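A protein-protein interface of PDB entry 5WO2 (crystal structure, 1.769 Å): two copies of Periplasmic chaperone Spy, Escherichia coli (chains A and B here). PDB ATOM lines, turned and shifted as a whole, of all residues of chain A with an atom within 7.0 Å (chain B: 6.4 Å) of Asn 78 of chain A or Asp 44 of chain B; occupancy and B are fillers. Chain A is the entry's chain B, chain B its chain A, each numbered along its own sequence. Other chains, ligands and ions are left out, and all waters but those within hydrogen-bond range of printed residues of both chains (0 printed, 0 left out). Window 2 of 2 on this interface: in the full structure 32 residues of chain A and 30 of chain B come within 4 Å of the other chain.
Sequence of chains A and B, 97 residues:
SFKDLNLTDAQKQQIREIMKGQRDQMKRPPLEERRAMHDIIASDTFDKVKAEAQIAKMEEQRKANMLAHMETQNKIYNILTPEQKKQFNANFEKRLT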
ATOM      1  N   THR A  72      -5.143   2.330  12.855  1.00  0.00           N
ATOM      2  CA  THR A  72      -6.320   3.113  12.483  1.00  0.00           C
ATOM      3  C   THR A  72      -6.045   3.951  11.234  1.00  0.00           C
ATOM      4  O   THR A  72      -6.837   3.939  10.302  1.00  0.00           O
ATOM      5  CB  THR A  72      -6.761   4.007  13.665  1.00  0.00           C
ATOM      6  OG1 THR A  72      -7.137   3.162  14.760  1.00  0.00           O
ATOM      7  CG2 THR A  72      -7.945   4.862  13.320  1.00  0.00           C
ATOM      8  N   GLN A  73      -4.923   4.659  11.200  1.00  0.00           N
ATOM      9  CA  GLN A  73      -4.601   5.463  10.032  1.00  0.00           C
ATOM     10  C   GLN A  73      -4.391   4.614   8.776  1.00  0.00           C
ATOM     11  O   GLN A  73      -4.762   5.007   7.666  1.00  0.00           O
ATOM     12  CB  GLN A  73      -3.364   6.291  10.300  1.00  0.00           C
ATOM     13  CG  GLN A  73      -3.591   7.319  11.426  1.00  0.00           C
ATOM     14  CD  GLN A  73      -4.587   8.363  11.030  1.00  0.00           C
ATOM     15  OE1 GLN A  73      -4.438   9.004   9.989  1.00  0.00           O
ATOM     16  NE2 GLN A  73      -5.636   8.518  11.827  1.00  0.00           N
ATOM     17  N   ASN A  74      -3.776   3.447   8.944  1.00  0.00           N
ATOM     18  CA  ASN A  74      -3.633   2.511   7.834  1.00  0.00           C
ATOM     19  C   ASN A  74      -5.005   2.066   7.326  1.00  0.00           C
ATOM     20  O   ASN A  74      -5.230   1.958   6.123  1.00  0.00           O
ATOM     21  CB  ASN A  74      -2.799   1.297   8.270  1.00  0.00           C
ATOM     22  CG  ASN A  74      -2.591   0.306   7.169  1.00  0.00           C
ATOM     23  OD1 ASN A  74      -3.396  -0.619   6.979  1.00  0.00           O
ATOM     24  ND2 ASN A  74      -1.518   0.486   6.412  1.00  0.00           N
ATOM     25  N   LYS A  75      -5.929   1.809   8.241  1.00  0.00           N
ATOM     26  CA  LYS A  75      -7.242   1.334   7.803  1.00  0.00           C
ATOM     27  C   LYS A  75      -7.937   2.438   7.010  1.00  0.00           C
ATOM     28  O   LYS A  75      -8.641   2.183   6.039  1.00  0.00           O
ATOM     29  CB  LYS A  75      -8.092   0.901   8.994  1.00  0.00           C
ATOM     30  CG  LYS A  75      -7.748  -0.499   9.514  1.00  0.00           C
ATOM     31  CD  LYS A  75      -8.682  -0.939  10.648  1.00  0.00           C
ATOM     32  CE  LYS A  75      -8.115  -2.111  11.397  1.00  0.00           C
ATOM     33  NZ  LYS A  75      -7.580  -3.168  10.479  1.00  0.00           N
ATOM     34  N   ILE A  76      -7.726   3.677   7.418  1.00  0.00           N
ATOM     35  CA  ILE A  76      -8.327   4.809   6.736  1.00  0.00           C
ATOM     36  C   ILE A  76      -7.716   4.982   5.351  1.00  0.00           C
ATOM     37  O   ILE A  76      -8.425   5.059   4.345  1.00  0.00           O
ATOM     38  CB  ILE A  76      -8.143   6.083   7.573  1.00  0.00           C
ATOM     39  CG1 ILE A  76      -9.036   5.999   8.818  1.00  0.00           C
ATOM     40  CG2 ILE A  76      -8.459   7.336   6.749  1.00  0.00           C
ATOM     41  CD1 ILE A  76      -8.872   7.114   9.762  1.00  0.00           C
ATOM     42  N   TYR A  77      -6.392   5.039   5.297  1.00  0.00           N
ATOM     43  CA  TYR A  77      -5.678   5.170   4.040  1.00  0.00           C
ATOM     44  C   TYR A  77      -6.247   4.192   3.005  1.00  0.00           C
ATOM     45  O   TYR A  77      -6.428   4.546   1.853  1.00  0.00           O
ATOM     46  CB  TYR A  77      -4.192   4.898   4.261  1.00  0.00           C
ATOM     47  CG  TYR A  77      -3.338   5.100   3.027  1.00  0.00           C
ATOM     48  CD1 TYR A  77      -2.961   6.374   2.630  1.00  0.00           C
ATOM     49  CD2 TYR A  77      -2.895   4.023   2.268  1.00  0.00           C
ATOM     50  CE1 TYR A  77      -2.192   6.581   1.499  1.00  0.00           C
ATOM     51  CE2 TYR A  77      -2.095   4.228   1.119  1.00  0.00           C
ATOM     52  CZ  TYR A  77      -1.738   5.505   0.770  1.00  0.00           C
ATOM     53  OH  TYR A  77      -0.946   5.766  -0.308  1.00  0.00           O
ATOM     54  N   ASN A  78      -6.554   2.979   3.435  1.00  0.00           N
ATOM     55  CA  ASN A  78      -7.003   1.960   2.483  1.00  0.00           C
ATOM     56  C   ASN A  78      -8.489   2.000   2.133  1.00  0.00           C
ATOM     57  O   ASN A  78      -8.927   1.250   1.269  1.00  0.00           O
ATOM     58  CB  ASN A  78      -6.628   0.590   3.005  1.00  0.00           C
ATOM     59  CG  ASN A  78      -5.187   0.275   2.742  1.00  0.00           C
ATOM     60  OD1 ASN A  78      -4.803   0.121   1.581  1.00  0.00           O
ATOM     61  ND2 ASN A  78      -4.362   0.195   3.810  1.00  0.00           N
ATOM     62  N   ILE A  79      -9.274   2.882   2.745  1.00  0.00           N
ATOM     63  CA  ILE A  79     -10.618   3.119   2.195  1.00  0.00           C
ATOM     64  C   ILE A  79     -10.613   4.223   1.143  1.00  0.00           C
ATOM     65  O   ILE A  79     -11.652   4.526   0.579  1.00  0.00           O
ATOM     66  CB  ILE A  79     -11.662   3.504   3.273  1.00  0.00           C
ATOM     67  CG1 ILE A  79     -11.392   4.876   3.878  1.00  0.00           C
ATOM     68  CG2 ILE A  79     -11.721   2.466   4.349  1.00  0.00           C
ATOM     69  CD1 ILE A  79     -12.550   5.434   4.658  1.00  0.00           C
ATOM     70  N   LEU A  80      -9.457   4.842   0.889  1.00  0.00           N
ATOM     71  CA  LEU A  80      -9.383   6.009  -0.004  1.00  0.00           C
ATOM     72  C   LEU A  80      -9.165   5.706  -1.484  1.00  0.00           C
ATOM     73  O   LEU A  80      -8.553   4.697  -1.830  1.00  0.00           O
ATOM     74  CB  LEU A  80      -8.244   6.937   0.434  1.00  0.00           C
ATOM     75  CG  LEU A  80      -8.265   7.539   1.847  1.00  0.00           C
ATOM     76  CD1 LEU A  80      -6.985   8.350   2.088  1.00  0.00           C
ATOM     77  CD2 LEU A  80      -9.495   8.381   2.068  1.00  0.00           C
ATOM     78  N   THR A  81      -9.654   6.606  -2.350  1.00  0.00           N
ATOM     79  CA  THR A  81      -9.347   6.559  -3.787  1.00  0.00           C
ATOM     80  C   THR A  81      -7.898   6.932  -4.073  1.00  0.00           C
ATOM     81  O   THR A  81      -7.280   7.631  -3.281  1.00  0.00           O
ATOM     82  CB  THR A  81     -10.210   7.524  -4.579  1.00  0.00           C
ATOM     83  OG1 THR A  81      -9.840   8.864  -4.236  1.00  0.00           O
ATOM     84  CG2 THR A  81     -11.692   7.297  -4.292  1.00  0.00           C
ATOM     85  N   LYS A  85      -5.569   9.278  -1.736  1.00  0.00           N
ATOM     86  CA  LYS A  85      -4.316   8.837  -1.106  1.00  0.00           C
ATOM     87  C   LYS A  85      -3.160   9.797  -1.418  1.00  0.00           C
ATOM     88  O   LYS A  85      -2.333  10.078  -0.569  1.00  0.00           O
ATOM     89  CB  LYS A  85      -3.923   7.438  -1.578  1.00  0.00           C
ATOM     90  CG  LYS A  85      -4.800   6.313  -1.108  1.00  0.00           C
ATOM     91  CD  LYS A  85      -4.383   4.975  -1.763  1.00  0.00           C
ATOM     92  CE  LYS A  85      -5.241   3.832  -1.232  1.00  0.00           C
ATOM     93  NZ  LYS A  85      -5.117   2.590  -2.028  1.00  0.00           N
ATOM     94  N   ILE B  41       2.049   3.377   7.400  1.00  0.00           N
ATOM     95  CA  ILE B  41       0.672   3.797   7.274  1.00  0.00           C
ATOM     96  C   ILE B  41       0.192   3.722   5.814  1.00  0.00           C
ATOM     97  O   ILE B  41      -0.909   3.253   5.587  1.00  0.00           O
ATOM     98  CB  ILE B  41       0.464   5.222   7.810  1.00  0.00           C
ATOM     99  CG1 ILE B  41       0.442   5.192   9.334  1.00  0.00           C
ATOM    100  CG2 ILE B  41      -0.848   5.803   7.287  1.00  0.00           C
ATOM    101  CD1 ILE B  41       0.470   6.561   9.973  1.00  0.00           C
ATOM    102  N   ALA B  42       1.017   4.134   4.855  1.00  0.00           N
ATOM    103  CA  ALA B  42       0.593   4.199   3.473  1.00  0.00           C
ATOM    104  C   ALA B  42       0.913   2.894   2.762  1.00  0.00           C
ATOM    105  O   ALA B  42       1.738   2.866   1.866  1.00  0.00           O
ATOM    106  CB  ALA B  42       1.275   5.316   2.756  1.00  0.00           C
ATOM    107  N   SER B  43       0.263   1.819   3.150  1.00  0.00           N
ATOM    108  CA  SER B  43       0.608   0.498   2.610  1.00  0.00           C
ATOM    109  C   SER B  43      -0.681  -0.265   2.546  1.00  0.00           C
ATOM    110  O   SER B  43      -1.595   0.058   3.305  1.00  0.00           O
ATOM    111  CB  SER B  43       1.654  -0.179   3.526  1.00  0.00           C
ATOM    112  OG  SER B  43       1.740  -1.580   3.282  1.00  0.00           O
ATOM    113  N   ASP B  44      -0.812  -1.278   1.679  1.00  0.00           N
ATOM    114  CA  ASP B  44      -2.132  -1.896   1.572  1.00  0.00           C
ATOM    115  C   ASP B  44      -2.385  -2.935   2.687  1.00  0.00           C
ATOM    116  O   ASP B  44      -3.446  -3.570   2.714  1.00  0.00           O
ATOM    117  CB  ASP B  44      -2.400  -2.485   0.123  1.00  0.00           C
ATOM    118  CG  ASP B  44      -1.457  -3.683  -0.305  1.00  0.00           C
ATOM    119  OD1 ASP B  44      -0.617  -4.086   0.500  1.00  0.00           O
ATOM    120  OD2 ASP B  44      -1.542  -4.259  -1.456  1.00  0.00           O
ATOM    121  N   THR B  45      -1.426  -3.110   3.599  1.00  0.00           N
ATOM    122  CA  THR B  45      -1.616  -3.959   4.781  1.00  0.00           C
ATOM    123  C   THR B  45      -0.951  -3.319   5.982  1.00  0.00           C
ATOM    124  O   THR B  45      -0.036  -2.503   5.825  1.00  0.00           O
ATOM    125  CB  THR B  45      -1.006  -5.365   4.596  1.00  0.00           C
ATOM    126  OG1 THR B  45       0.427  -5.247   4.527  1.00  0.00           O
ATOM    127  CG2 THR B  45      -1.540  -6.019   3.332  1.00  0.00           C
ATOM    128  N   PHE B  46      -1.390  -3.678   7.182  1.00  0.00           N
ATOM    129  CA  PHE B  46      -0.747  -3.149   8.380  1.00  0.00           C
ATOM    130  C   PHE B  46       0.243  -4.159   8.946  1.00  0.00           C
ATOM    131  O   PHE B  46      -0.149  -5.231   9.372  1.00  0.00           O
ATOM    132  CB  PHE B  46      -1.778  -2.805   9.427  1.00  0.00           C
ATOM    133  CG  PHE B  46      -1.174  -2.246  10.682  1.00  0.00           C
ATOM    134  CD1 PHE B  46      -0.508  -1.021  10.689  1.00  0.00           C
ATOM    135  CD2 PHE B  46      -1.241  -2.994  11.835  1.00  0.00           C
ATOM    136  CE1 PHE B  46       0.069  -0.560  11.922  1.00  0.00           C
ATOM    137  CE2 PHE B  46      -0.678  -2.545  13.011  1.00  0.00           C
ATOM    138  CZ  PHE B  46      -0.054  -1.389  13.042  1.00  0.00           C
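The backbone carbonyl oxygen of Ser 43 of chain B sits at hydrogen-bond distance from the side-chain amide nitrogen of Asn 74 of chain A, at 3.1 Å. The backbone carbonyl oxygen of Thr 45 of chain B is in hydrogen-bond range of the side-chain amide nitrogen of Asn 74 of chain A (3.4 Å). O of Ser 43 of chain B sits at hydrogen-bond distance from ND2 of Asn 78 of chain A, 2.8 Å away. The backbone carbonyl oxygen (O) of Ile 41 of chain B is in hydrogen-bond range of the side-chain amide nitrogen (ND2) of Asn 74 of chain A, 3.0 Å away.
The side-chain hydroxyl of Ser 43 of chain B sits at hydrogen-bond distance from the backbone carbonyl oxygen of Thr 45 of chain B, 3.2 Å away. The backbone carbonyl oxygen (O) of Asn 74 of chain A is in hydrogen-bond range of the side-chain amide nitrogen (ND2) of Asn 78 of chain A, at 3.0 Å.
Gln 73 of chain A touches Ile 41 of chain B. Asn 74 of chain A touches Phe 46 of chain B. O of Ile 41 of chain B touches CB of Tyr 77 of chain A (3.9 Å). Ala 42 of chain B touches Tyr 77 of chain A. N of Ser 43 of chain B touches CE2 of Tyr 77 of chain A (3.9 Å). CA of Asp 44 of chain B touches OD1 of Asn 78 of chain A, 3.3 Å away.
Printed residues of chain B within 4 Å of Asn 78 of chain A: Ser 43 and Asp 44. Asp 44 of chain B touches just one residue of chain A: Asn 78 (3.3 Å). Of the printed residues of chain A, Phe 46 of chain B touches Asn 74. Of the printed residues of chain B, Gln 73 of chain A touches Ile 41 (3.9 Å). Printed residues of chain A within 4 Å of Thr 45 of chain B: Asn 74 (3.4 Å). Of the printed residues of chain B, Asn 74 of chain A touches Ile 41 (3.0 Å), Ser 43 (3.1 Å), Thr 45 (3.4 Å) and Phe 46 (3.7 Å). Thr 72 of chain A touches none of the printed residues of chain B. Lys 75 of chain A touches none of the printed residues of chain B. The nearest residue of chain A that does not touch Asp 44 of chain B is Asn 74 of chain A (5.0 Å).
Of the 6 printed residues of chain B, 6 touch a printed residue of chain A. Along chain A the printed residues that touch a printed residue of chain B span positions 73 to 78. Among the printed residues, no Asp or Glu carboxylate lies within 4 Å of a Lys or Arg side-chain nitrogen of the other chain.
No position is printed for both chains. Of the 10 pairs that touch across the chains among the printed residues, none has its exchanged pair printed and touching as well.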
